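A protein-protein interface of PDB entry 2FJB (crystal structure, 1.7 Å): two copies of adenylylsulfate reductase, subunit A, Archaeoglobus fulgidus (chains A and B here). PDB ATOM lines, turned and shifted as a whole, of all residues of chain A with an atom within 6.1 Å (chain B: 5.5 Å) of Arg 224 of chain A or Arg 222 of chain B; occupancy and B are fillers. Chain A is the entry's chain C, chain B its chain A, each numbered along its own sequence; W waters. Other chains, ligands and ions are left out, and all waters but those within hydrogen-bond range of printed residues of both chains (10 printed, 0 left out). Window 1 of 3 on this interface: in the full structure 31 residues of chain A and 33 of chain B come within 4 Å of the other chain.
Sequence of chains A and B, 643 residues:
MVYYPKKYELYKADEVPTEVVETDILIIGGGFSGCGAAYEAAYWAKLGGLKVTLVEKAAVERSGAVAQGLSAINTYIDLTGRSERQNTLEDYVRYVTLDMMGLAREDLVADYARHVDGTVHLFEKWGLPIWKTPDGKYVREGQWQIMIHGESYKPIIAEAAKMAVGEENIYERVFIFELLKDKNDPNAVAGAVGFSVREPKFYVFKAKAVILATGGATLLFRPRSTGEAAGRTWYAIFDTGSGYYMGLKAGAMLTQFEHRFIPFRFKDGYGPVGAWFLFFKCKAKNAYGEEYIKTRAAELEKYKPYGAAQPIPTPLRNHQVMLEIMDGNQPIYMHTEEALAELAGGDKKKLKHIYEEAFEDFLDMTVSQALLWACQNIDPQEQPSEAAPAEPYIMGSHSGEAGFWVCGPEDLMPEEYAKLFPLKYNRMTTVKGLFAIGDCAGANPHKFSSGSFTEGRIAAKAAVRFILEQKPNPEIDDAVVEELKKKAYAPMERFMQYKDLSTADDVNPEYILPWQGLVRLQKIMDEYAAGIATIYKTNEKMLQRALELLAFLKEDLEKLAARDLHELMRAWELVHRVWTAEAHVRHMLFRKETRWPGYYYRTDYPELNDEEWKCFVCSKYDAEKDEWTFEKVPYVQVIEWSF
O of Arg 224 of chain A sits at hydrogen-bond distance from NH1 of Arg 222 of chain B, 2.8 Å away.
The backbone carbonyl oxygen (O) of Arg 224 of chain B is in hydrogen-bond range of the guanidinium group (NH1) of Arg 222 of chain A, 2.8 Å away.
The side-chain amino group (NZ) of Lys 523 of chain B sits at hydrogen-bond distance from the backbone carbonyl oxygen (O) of Arg 224 of chain A (3.0 Å).
The side-chain amino group of Lys 523 of chain B lies within hydrogen-bond range of the side-chain hydroxyl of Ser 225 of chain A, 2.8 Å away.
OD2 of Asp 268 of chain A is in salt-bridge range of NZ of Lys 523 of chain B, at 2.8 Å.
The side-chain carboxylate (OE1) of Glu 527 of chain B is in salt-bridge range of the side-chain amino group (NZ) of Lys 267 of chain A (2.7 Å).
The side-chain carboxylate of Glu 527 of chain B lies close to the backbone carbonyl oxygen of Arg 224 of chain A, 3.5 Å away.
The backbone NH (N) of Arg 222 of chain B sits at hydrogen-bond distance from the backbone carbonyl oxygen (O) of Gln 522 of chain B.
NH2 of Arg 222 of chain B is in salt-bridge range of OD2 of Asp 526 of chain B, 2.8 Å away.
NH2 of Arg 222 of chain B is in salt-bridge range of OE2 of Glu 527 of chain B (3.3 Å).
NE of Arg 224 of chain A lies within hydrogen-bond range of O of Pro 389 of chain A (2.6 Å).
NH2 of Arg 224 of chain A is in hydrogen-bond range of OH of Tyr 536 of chain A (3.1 Å).
OD1 of Asp 268 of chain A lies within salt-bridge range of NZ of Lys 267 of chain A (2.9 Å).
Among the printed residues, merely in contact across the chains: Thr 226 of chain A with Thr 226 of chain B (3.6 Å), Ser 225 of chain A with Arg 222 of chain B (3.8 Å), Thr 226 of chain A with Arg 222 of chain B (3.9 Å) and Arg 222 of chain A with Thr 226 of chain B (3.9 Å).
Pro 223 of chain A touches none of the printed residues of chain B.
Arg 224 of chain A touches just these residues of chain B: Arg 222, Lys 523 and Glu 527.
Of the printed residues of chain B, Thr 226 of chain A touches Arg 222 and Thr 226.
Printed residues of chain B within 4 Å of Asp 268 of chain A: Lys 523 (2.8 Å).
Of the printed residues of chain A, Arg 222 of chain B touches Arg 224, Ser 225 and Thr 226.
Printed residues of chain A within 4 Å of Arg 224 of chain B: Arg 222 (2.8 Å).
Of the printed residues of chain A, Lys 523 of chain B touches Arg 224 (3.0 Å), Ser 225 (2.8 Å) and Asp 268 (2.8 Å).
The nearest printed residue of chain B that does not touch Arg 224 of chain A is Ala 533 of chain B (5.6 Å).
Of the 13 printed residues of chain B, 5 touch a printed residue of chain A.
Among the printed residues, 11 pairs touch across the chains.
Arg 222 of chain A touches Arg 224 of chain B, and with the chains exchanged Arg 224 of chain A touches Arg 222 of chain B.
Arg 222 of chain A touches Thr 226 of chain B, and with the chains exchanged Thr 226 of chain A touches Arg 222 of chain B.
Thr 226 of chain B touches its own counterpart, Thr 226 of chain A.
Positions printed for both chains: 222, 223, 224, 226, 391 and 532.
Of the 11 pairs that touch across the chains among the printed residues, 5 have their exchanged pair printed and touching as well.
Water W1 bridges NH1 of Arg 224 of chain A (2.6 Å) and O of Ala 533 of chain B (3.0 Å).
Water W6 lies within hydrogen-bond range of the backbone carbonyl oxygen (O) of Pro 223 of chain A (2.7 Å), the guanidinium group (NH1) of Arg 222 of chain B (3.1 Å) and the backbone carbonyl oxygen (O) of Arg 224 of chain A (3.5 Å).
Water W4 lies within hydrogen-bond range of the backbone NH (N) of Thr 226 of chain A (2.9 Å) and the guanidinium group (NH1) of Arg 222 of chain B (3.2 Å).
Water W5 bridges the backbone carbonyl oxygen of Thr 226 of chain B (2.9 Å) and the backbone carbonyl oxygen of Thr 226 of chain A (3.1 Å).
Water W10 bridges OE2 of Glu 527 of chain B and OD2 of Asp 268 of chain A.
Water W7 bridges OE1 of Gln 522 of chain B (3.1 Å) and OG1 of Thr 226 of chain A (3.3 Å).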
ATOM      1  N   ARG A 222     -31.506 -34.276  -3.970  1.00  0.00           N
ATOM      2  CA  ARG A 222     -31.644 -33.431  -5.148  1.00  0.00           C
ATOM      3  C   ARG A 222     -30.266 -32.832  -5.462  1.00  0.00           C
ATOM      4  O   ARG A 222     -29.599 -32.295  -4.576  1.00  0.00           O
ATOM      5  CB  ARG A 222     -32.665 -32.323  -4.864  1.00  0.00           C
ATOM      6  CG  ARG A 222     -32.834 -31.307  -5.983  1.00  0.00           C
ATOM      7  CD  ARG A 222     -34.230 -30.689  -5.957  1.00  0.00           C
ATOM      8  NE  ARG A 222     -34.562 -30.123  -4.654  1.00  0.00           N
ATOM      9  CZ  ARG A 222     -35.770 -29.681  -4.314  1.00  0.00           C
ATOM     10  NH1 ARG A 222     -36.772 -29.738  -5.183  1.00  0.00           N
ATOM     11  NH2 ARG A 222     -35.979 -29.188  -3.102  1.00  0.00           N
ATOM     12  N   PRO A 223     -29.813 -32.942  -6.723  1.00  0.00           N
ATOM     13  CA  PRO A 223     -28.512 -32.414  -7.161  1.00  0.00           C
ATOM     14  C   PRO A 223     -28.571 -30.902  -7.390  1.00  0.00           C
ATOM     15  O   PRO A 223     -29.635 -30.296  -7.277  1.00  0.00           O
ATOM     16  CB  PRO A 223     -28.249 -33.166  -8.471  1.00  0.00           C
ATOM     17  CG  PRO A 223     -29.158 -34.364  -8.403  1.00  0.00           C
ATOM     18  CD  PRO A 223     -30.389 -33.812  -7.759  1.00  0.00           C
ATOM     19  N   ARG A 224     -27.434 -30.299  -7.726  1.00  0.00           N
ATOM     20  CA  ARG A 224     -27.404 -28.861  -7.968  1.00  0.00           C
ATOM     21  C   ARG A 224     -27.949 -28.497  -9.348  1.00  0.00           C
ATOM     22  O   ARG A 224     -28.137 -27.329  -9.661  1.00  0.00           O
ATOM     23  CB  ARG A 224     -25.989 -28.313  -7.765  1.00  0.00           C
ATOM     24  CG  ARG A 224     -25.609 -28.235  -6.287  1.00  0.00           C
ATOM     25  CD  ARG A 224     -24.315 -27.472  -6.043  1.00  0.00           C
ATOM     26  NE  ARG A 224     -24.014 -27.391  -4.613  1.00  0.00           N
ATOM     27  CZ  ARG A 224     -24.746 -26.719  -3.728  1.00  0.00           C
ATOM     28  NH1 ARG A 224     -25.823 -26.055  -4.124  1.00  0.00           N
ATOM     29  NH2 ARG A 224     -24.412 -26.720  -2.442  1.00  0.00           N
ATOM     30  N   SER A 225     -28.193 -29.510 -10.171  1.00  0.00           N
ATOM     31  CA  SER A 225     -28.783 -29.305 -11.492  1.00  0.00           C
ATOM     32  C   SER A 225     -29.918 -30.313 -11.546  1.00  0.00           C
ATOM     33  O   SER A 225     -29.720 -31.496 -11.261  1.00  0.00           O
ATOM     34  CB  SER A 225     -27.761 -29.549 -12.603  1.00  0.00           C
ATOM     35  OG  SER A 225     -26.771 -28.535 -12.587  1.00  0.00           O
ATOM     36  N   THR A 226     -31.107 -29.846 -11.910  1.00  0.00           N
ATOM     37  CA  THR A 226     -32.288 -30.700 -11.917  1.00  0.00           C
ATOM     38  C   THR A 226     -32.921 -31.079 -13.250  1.00  0.00           C
ATOM     39  O   THR A 226     -33.914 -31.804 -13.267  1.00  0.00           O
ATOM     40  CB  THR A 226     -33.377 -30.070 -11.044  1.00  0.00           C
ATOM     41  OG1 THR A 226     -33.673 -28.759 -11.536  1.00  0.00           O
ATOM     42  CG2 THR A 226     -32.903 -29.957  -9.604  1.00  0.00           C
ATOM     43  N   LYS A 267     -17.457 -26.705  -9.936  1.00  0.00           N
ATOM     44  CA  LYS A 267     -18.897 -26.503 -10.039  1.00  0.00           C
ATOM     45  C   LYS A 267     -19.558 -27.024 -11.312  1.00  0.00           C
ATOM     46  O   LYS A 267     -18.994 -26.937 -12.406  1.00  0.00           O
ATOM     47  CB  LYS A 267     -19.223 -25.015  -9.867  1.00  0.00           C
ATOM     48  CG  LYS A 267     -20.714 -24.685  -9.862  1.00  0.00           C
ATOM     49  CD  LYS A 267     -20.950 -23.187  -9.641  1.00  0.00           C
ATOM     50  CE  LYS A 267     -22.438 -22.839  -9.660  1.00  0.00           C
ATOM     51  NZ  LYS A 267     -23.058 -23.087 -10.995  1.00  0.00           N
ATOM     52  N   ASP A 268     -20.756 -27.581 -11.130  1.00  0.00           N
ATOM     53  CA  ASP A 268     -21.594 -28.110 -12.205  1.00  0.00           C
ATOM     54  C   ASP A 268     -21.110 -29.374 -12.906  1.00  0.00           C
ATOM     55  O   ASP A 268     -21.868 -30.340 -13.028  1.00  0.00           O
ATOM     56  CB  ASP A 268     -21.863 -27.004 -13.229  1.00  0.00           C
ATOM     57  CG  ASP A 268     -22.746 -25.898 -12.668  1.00  0.00           C
ATOM     58  OD1 ASP A 268     -22.817 -24.818 -13.284  1.00  0.00           O
ATOM     59  OD2 ASP A 268     -23.374 -26.112 -11.610  1.00  0.00           O
ATOM     60  N   TYR A 270     -18.489 -31.050 -11.837  1.00  0.00           N
ATOM     61  CA  TYR A 270     -17.967 -31.857 -10.739  1.00  0.00           C
ATOM     62  C   TYR A 270     -16.635 -32.536 -10.993  1.00  0.00           C
ATOM     63  O   TYR A 270     -16.376 -33.640 -10.496  1.00  0.00           O
ATOM     64  CB  TYR A 270     -19.023 -32.875 -10.305  1.00  0.00           C
ATOM     65  CG  TYR A 270     -20.188 -32.187  -9.647  1.00  0.00           C
ATOM     66  CD1 TYR A 270     -21.497 -32.569  -9.915  1.00  0.00           C
ATOM     67  CD2 TYR A 270     -19.975 -31.106  -8.786  1.00  0.00           C
ATOM     68  CE1 TYR A 270     -22.573 -31.886  -9.348  1.00  0.00           C
ATOM     69  CE2 TYR A 270     -21.036 -30.422  -8.213  1.00  0.00           C
ATOM     70  CZ  TYR A 270     -22.330 -30.812  -8.497  1.00  0.00           C
ATOM     71  OH  TYR A 270     -23.374 -30.118  -7.936  1.00  0.00           O
ATOM     72  N   ILE A 325     -19.670 -19.899   2.257  1.00  0.00           N
ATOM     73  CA  ILE A 325     -20.947 -19.941   1.560  1.00  0.00           C
ATOM     74  C   ILE A 325     -22.042 -19.301   2.414  1.00  0.00           C
ATOM     75  O   ILE A 325     -22.868 -18.537   1.913  1.00  0.00           O
ATOM     76  CB  ILE A 325     -21.336 -21.395   1.213  1.00  0.00           C
ATOM     77  CG1 ILE A 325     -20.343 -21.960   0.193  1.00  0.00           C
ATOM     78  CG2 ILE A 325     -22.756 -21.442   0.653  1.00  0.00           C
ATOM     79  CD1 ILE A 325     -20.505 -23.445  -0.077  1.00  0.00           C
ATOM     80  N   ALA A 388     -17.664 -25.903  -5.879  1.00  0.00           N
ATOM     81  CA  ALA A 388     -18.725 -25.937  -4.884  1.00  0.00           C
ATOM     82  C   ALA A 388     -18.940 -27.345  -4.351  1.00  0.00           C
ATOM     83  O   ALA A 388     -18.580 -28.327  -4.999  1.00  0.00           O
ATOM     84  CB  ALA A 388     -20.023 -25.414  -5.500  1.00  0.00           C
ATOM     85  N   PRO A 389     -19.506 -27.461  -3.141  1.00  0.00           N
ATOM     86  CA  PRO A 389     -19.745 -28.797  -2.593  1.00  0.00           C
ATOM     87  C   PRO A 389     -20.998 -29.343  -3.272  1.00  0.00           C
ATOM     88  O   PRO A 389     -21.942 -28.597  -3.515  1.00  0.00           O
ATOM     89  CB  PRO A 389     -19.954 -28.528  -1.106  1.00  0.00           C
ATOM     90  CG  PRO A 389     -20.595 -27.176  -1.098  1.00  0.00           C
ATOM     91  CD  PRO A 389     -19.793 -26.417  -2.139  1.00  0.00           C
ATOM     92  N   ALA A 390     -21.001 -30.628  -3.609  1.00  0.00           N
ATOM     93  CA  ALA A 390     -22.167 -31.217  -4.256  1.00  0.00           C
ATOM     94  C   ALA A 390     -23.135 -31.723  -3.188  1.00  0.00           C
ATOM     95  O   ALA A 390     -22.927 -31.498  -1.997  1.00  0.00           O
ATOM     96  CB  ALA A 390     -21.739 -32.365  -5.162  1.00  0.00           C
ATOM     97  N   GLU A 391     -24.195 -32.401  -3.616  1.00  0.00           N
ATOM     98  CA  GLU A 391     -25.167 -32.946  -2.676  1.00  0.00           C
ATOM     99  C   GLU A 391     -24.556 -34.187  -2.014  1.00  0.00           C
ATOM    100  O   GLU A 391     -23.518 -34.686  -2.451  1.00  0.00           O
ATOM    101  CB  GLU A 391     -26.469 -33.316  -3.397  1.00  0.00           C
ATOM    102  CG  GLU A 391     -26.385 -34.583  -4.231  1.00  0.00           C
ATOM    103  CD  GLU A 391     -25.779 -34.364  -5.610  1.00  0.00           C
ATOM    104  OE1 GLU A 391     -25.159 -33.305  -5.852  1.00  0.00           O
ATOM    105  OE2 GLU A 391     -25.925 -35.269  -6.456  1.00  0.00           O
ATOM    106  N   ILE A 532     -28.554 -29.904   0.120  1.00  0.00           N
ATOM    107  CA  ILE A 532     -28.085 -28.587  -0.299  1.00  0.00           C
ATOM    108  C   ILE A 532     -29.064 -27.463   0.038  1.00  0.00           C
ATOM    109  O   ILE A 532     -28.645 -26.328   0.278  1.00  0.00           O
ATOM    110  CB  ILE A 532     -27.811 -28.538  -1.822  1.00  0.00           C
ATOM    111  CG1 ILE A 532     -29.120 -28.733  -2.595  1.00  0.00           C
ATOM    112  CG2 ILE A 532     -26.790 -29.598  -2.198  1.00  0.00           C
ATOM    113  CD1 ILE A 532     -28.964 -28.694  -4.104  1.00  0.00           C
ATOM    114  N   TYR A 536     -26.735 -28.129   4.187  1.00  0.00           N
ATOM    115  CA  TYR A 536     -26.403 -29.320   4.957  1.00  0.00           C
ATOM    116  C   TYR A 536     -26.727 -29.296   6.455  1.00  0.00           C
ATOM    117  O   TYR A 536     -26.073 -29.981   7.247  1.00  0.00           O
ATOM    118  CB  TYR A 536     -24.922 -29.657   4.741  1.00  0.00           C
ATOM    119  CG  TYR A 536     -24.491 -29.539   3.291  1.00  0.00           C
ATOM    120  CD1 TYR A 536     -23.888 -28.373   2.817  1.00  0.00           C
ATOM    121  CD2 TYR A 536     -24.730 -30.571   2.384  1.00  0.00           C
ATOM    122  CE1 TYR A 536     -23.536 -28.236   1.479  1.00  0.00           C
ATOM    123  CE2 TYR A 536     -24.382 -30.442   1.040  1.00  0.00           C
ATOM    124  CZ  TYR A 536     -23.786 -29.269   0.597  1.00  0.00           C
ATOM    125  OH  TYR A 536     -23.442 -29.119  -0.727  1.00  0.00           O
ATOM    126  N   LEU B 220     -38.589 -17.497 -13.524  1.00  0.00           N
ATOM    127  CA  LEU B 220     -37.280 -16.948 -13.874  1.00  0.00           C
ATOM    128  C   LEU B 220     -36.283 -17.674 -12.970  1.00  0.00           C
ATOM    129  O   LEU B 220     -35.150 -17.959 -13.367  1.00  0.00           O
ATOM    130  CB  LEU B 220     -37.200 -15.450 -13.569  1.00  0.00           C
ATOM    131  CG  LEU B 220     -37.399 -14.475 -14.730  1.00  0.00           C
ATOM    132  CD1 LEU B 220     -38.818 -14.576 -15.245  1.00  0.00           C
ATOM    133  CD2 LEU B 220     -37.091 -13.057 -14.261  1.00  0.00           C
ATOM    134  N   PHE B 221     -36.728 -17.955 -11.746  1.00  0.00           N
ATOM    135  CA  PHE B 221     -35.919 -18.639 -10.738  1.00  0.00           C
ATOM    136  C   PHE B 221     -36.352 -20.086 -10.530  1.00  0.00           C
ATOM    137  O   PHE B 221     -37.537 -20.411 -10.614  1.00  0.00           O
ATOM    138  CB  PHE B 221     -36.023 -17.932  -9.382  1.00  0.00           C
ATOM    139  CG  PHE B 221     -35.335 -16.598  -9.319  1.00  0.00           C
ATOM    140  CD1 PHE B 221     -35.930 -15.456  -9.852  1.00  0.00           C
ATOM    141  CD2 PHE B 221     -34.096 -16.480  -8.694  1.00  0.00           C
ATOM    142  CE1 PHE B 221     -35.297 -14.213  -9.758  1.00  0.00           C
ATOM    143  CE2 PHE B 221     -33.456 -15.241  -8.597  1.00  0.00           C
ATOM    144  CZ  PHE B 221     -34.056 -14.110  -9.128  1.00  0.00           C
ATOM    145  N   ARG B 222     -35.386 -20.948 -10.237  1.00  0.00           N
ATOM    146  CA  ARG B 222     -35.678 -22.351  -9.975  1.00  0.00           C
ATOM    147  C   ARG B 222     -36.580 -22.420  -8.739  1.00  0.00           C
ATOM    148  O   ARG B 222     -36.296 -21.790  -7.721  1.00  0.00           O
ATOM    149  CB  ARG B 222     -34.367 -23.113  -9.730  1.00  0.00           C
ATOM    150  CG  ARG B 222     -34.547 -24.562  -9.331  1.00  0.00           C
ATOM    151  CD  ARG B 222     -33.291 -25.375  -9.635  1.00  0.00           C
ATOM    152  NE  ARG B 222     -32.087 -24.756  -9.095  1.00  0.00           N
ATOM    153  CZ  ARG B 222     -30.853 -25.203  -9.314  1.00  0.00           C
ATOM    154  NH1 ARG B 222     -30.658 -26.277 -10.067  1.00  0.00           N
ATOM    155  NH2 ARG B 222     -29.815 -24.575  -8.781  1.00  0.00           N
ATOM    156  N   PRO B 223     -37.697 -23.166  -8.824  1.00  0.00           N
ATOM    157  CA  PRO B 223     -38.638 -23.307  -7.705  1.00  0.00           C
ATOM    158  C   PRO B 223     -38.154 -24.326  -6.675  1.00  0.00           C
ATOM    159  O   PRO B 223     -37.137 -24.988  -6.879  1.00  0.00           O
ATOM    160  CB  PRO B 223     -39.930 -23.777  -8.384  1.00  0.00           C
ATOM    161  CG  PRO B 223     -39.751 -23.403  -9.826  1.00  0.00           C
ATOM    162  CD  PRO B 223     -38.297 -23.675 -10.067  1.00  0.00           C
ATOM    163  N   ARG B 224     -38.895 -24.459  -5.579  1.00  0.00           N
ATOM    164  CA  ARG B 224     -38.527 -25.411  -4.538  1.00  0.00           C
ATOM    165  C   ARG B 224     -38.928 -26.837  -4.905  1.00  0.00           C
ATOM    166  O   ARG B 224     -38.589 -27.789  -4.208  1.00  0.00           O
ATOM    167  CB  ARG B 224     -39.138 -25.000  -3.201  1.00  0.00           C
ATOM    168  CG  ARG B 224     -38.478 -23.759  -2.610  1.00  0.00           C
ATOM    169  CD  ARG B 224     -38.920 -23.511  -1.183  1.00  0.00           C
ATOM    170  NE  ARG B 224     -38.278 -22.327  -0.616  1.00  0.00           N
ATOM    171  CZ  ARG B 224     -37.006 -22.263  -0.233  1.00  0.00           C
ATOM    172  NH1 ARG B 224     -36.215 -23.325  -0.349  1.00  0.00           N
ATOM    173  NH2 ARG B 224     -36.520 -21.130   0.263  1.00  0.00           N
ATOM    174  N   THR B 226     -38.935 -29.150  -8.482  1.00  0.00           N
ATOM    175  CA  THR B 226     -38.454 -29.111  -9.856  1.00  0.00           C
ATOM    176  C   THR B 226     -38.978 -30.158 -10.828  1.00  0.00           C
ATOM    177  O   THR B 226     -38.554 -30.189 -11.987  1.00  0.00           O
ATOM    178  CB  THR B 226     -36.922 -29.167  -9.860  1.00  0.00           C
ATOM    179  OG1 THR B 226     -36.488 -30.334  -9.149  1.00  0.00           O
ATOM    180  CG2 THR B 226     -36.352 -27.938  -9.163  1.00  0.00           C
ATOM    181  N   GLU B 391     -39.574 -19.150  -4.183  1.00  0.00           N
ATOM    182  CA  GLU B 391     -38.519 -18.488  -4.943  1.00  0.00           C
ATOM    183  C   GLU B 391     -39.021 -17.096  -5.343  1.00  0.00           C
ATOM    184  O   GLU B 391     -40.213 -16.797  -5.219  1.00  0.00           O
ATOM    185  CB  GLU B 391     -38.146 -19.307  -6.189  1.00  0.00           C
ATOM    186  CG  GLU B 391     -39.157 -19.250  -7.330  1.00  0.00           C
ATOM    187  CD  GLU B 391     -40.360 -20.162  -7.129  1.00  0.00           C
ATOM    188  OE1 GLU B 391     -40.508 -20.748  -6.038  1.00  0.00           O
ATOM    189  OE2 GLU B 391     -41.166 -20.289  -8.077  1.00  0.00           O
ATOM    190  N   GLN B 522     -33.328 -20.705 -15.032  1.00  0.00           N
ATOM    191  CA  GLN B 522     -33.665 -20.899 -13.625  1.00  0.00           C
ATOM    192  C   GLN B 522     -32.454 -21.219 -12.758  1.00  0.00           C
ATOM    193  O   GLN B 522     -32.355 -20.743 -11.626  1.00  0.00           O
ATOM    194  CB  GLN B 522     -34.734 -21.993 -13.482  1.00  0.00           C
ATOM    195  CG  GLN B 522     -36.090 -21.573 -14.053  1.00  0.00           C
ATOM    196  CD  GLN B 522     -37.104 -22.702 -14.100  1.00  0.00           C
ATOM    197  OE1 GLN B 522     -36.788 -23.855 -13.801  1.00  0.00           O
ATOM    198  NE2 GLN B 522     -38.333 -22.375 -14.490  1.00  0.00           N
ATOM    199  N   LYS B 523     -31.533 -22.020 -13.288  1.00  0.00           N
ATOM    200  CA  LYS B 523     -30.332 -22.385 -12.549  1.00  0.00           C
ATOM    201  C   LYS B 523     -29.437 -21.162 -12.359  1.00  0.00           C
ATOM    202  O   LYS B 523     -28.917 -20.925 -11.269  1.00  0.00           O
ATOM    203  CB  LYS B 523     -29.578 -23.494 -13.292  1.00  0.00           C
ATOM    204  CG  LYS B 523     -28.296 -23.956 -12.611  1.00  0.00           C
ATOM    205  CD  LYS B 523     -27.689 -25.139 -13.360  1.00  0.00           C
ATOM    206  CE  LYS B 523     -26.272 -25.440 -12.888  1.00  0.00           C
ATOM    207  NZ  LYS B 523     -26.214 -25.967 -11.502  1.00  0.00           N
ATOM    208  N   ASP B 526     -31.166 -18.781  -9.882  1.00  0.00           N
ATOM    209  CA  ASP B 526     -31.191 -19.386  -8.560  1.00  0.00           C
ATOM    210  C   ASP B 526     -29.827 -19.286  -7.869  1.00  0.00           C
ATOM    211  O   ASP B 526     -29.729 -18.888  -6.705  1.00  0.00           O
ATOM    212  CB  ASP B 526     -31.606 -20.857  -8.674  1.00  0.00           C
ATOM    213  CG  ASP B 526     -31.681 -21.548  -7.330  1.00  0.00           C
ATOM    214  OD1 ASP B 526     -32.140 -20.907  -6.361  1.00  0.00           O
ATOM    215  OD2 ASP B 526     -31.294 -22.734  -7.248  1.00  0.00           O
ATOM    216  N   GLU B 527     -28.774 -19.615  -8.606  1.00  0.00           N
ATOM    217  CA  GLU B 527     -27.429 -19.628  -8.043  1.00  0.00           C
ATOM    218  C   GLU B 527     -26.684 -18.303  -7.933  1.00  0.00           C
ATOM    219  O   GLU B 527     -25.817 -18.155  -7.070  1.00  0.00           O
ATOM    220  CB  GLU B 527     -26.579 -20.637  -8.822  1.00  0.00           C
ATOM    221  CG  GLU B 527     -27.234 -22.011  -8.883  1.00  0.00           C
ATOM    222  CD  GLU B 527     -26.425 -23.039  -9.643  1.00  0.00           C
ATOM    223  OE1 GLU B 527     -25.639 -22.656 -10.533  1.00  0.00           O
ATOM    224  OE2 GLU B 527     -26.598 -24.241  -9.359  1.00  0.00           O
ATOM    225  N   ILE B 532     -33.355 -19.164  -4.071  1.00  0.00           N
ATOM    226  CA  ILE B 532     -33.426 -20.000  -2.879  1.00  0.00           C
ATOM    227  C   ILE B 532     -32.095 -20.679  -2.556  1.00  0.00           C
ATOM    228  O   ILE B 532     -31.777 -20.908  -1.387  1.00  0.00           O
ATOM    229  CB  ILE B 532     -34.518 -21.087  -3.023  1.00  0.00           C
ATOM    230  CG1 ILE B 532     -34.169 -22.041  -4.171  1.00  0.00           C
ATOM    231  CG2 ILE B 532     -35.878 -20.428  -3.252  1.00  0.00           C
ATOM    232  CD1 ILE B 532     -35.207 -23.127  -4.408  1.00  0.00           C
ATOM    233  N   ALA B 533     -31.315 -20.983  -3.591  1.00  0.00           N
ATOM    234  CA  ALA B 533     -30.028 -21.660  -3.430  1.00  0.00           C
ATOM    235  C   ALA B 533     -29.106 -21.017  -2.394  1.00  0.00           C
ATOM    236  O   ALA B 533     -28.413 -21.714  -1.652  1.00  0.00           O
ATOM    237  CB  ALA B 533     -29.312 -21.734  -4.774  1.00  0.00           C
HETATM  238  O   HOH W   1     -27.257 -24.247  -2.841  1.00  0.00           O
HETATM  239  O   HOH W   2     -26.875 -25.060  -6.569  1.00  0.00           O
HETATM  240  O   HOH W   3     -38.951 -31.350  -6.590  1.00  0.00           O
HETATM  241  O   HOH W   4     -30.848 -27.254 -13.073  1.00  0.00           O
HETATM  242  O   HOH W   5     -36.228 -29.766 -13.684  1.00  0.00           O
HETATM  243  O   HOH W   6     -30.671 -27.762  -7.299  1.00  0.00           O
HETATM  244  O   HOH W   7     -35.635 -26.146 -12.125  1.00  0.00           O
HETATM  245  O   HOH W   8     -36.349 -32.377 -11.457  1.00  0.00           O
HETATM  246  O   HOH W   9     -35.345 -26.832  -5.651  1.00  0.00           O
HETATM  247  O   HOH W  10     -24.084 -25.482  -8.400  1.00  0.00           O
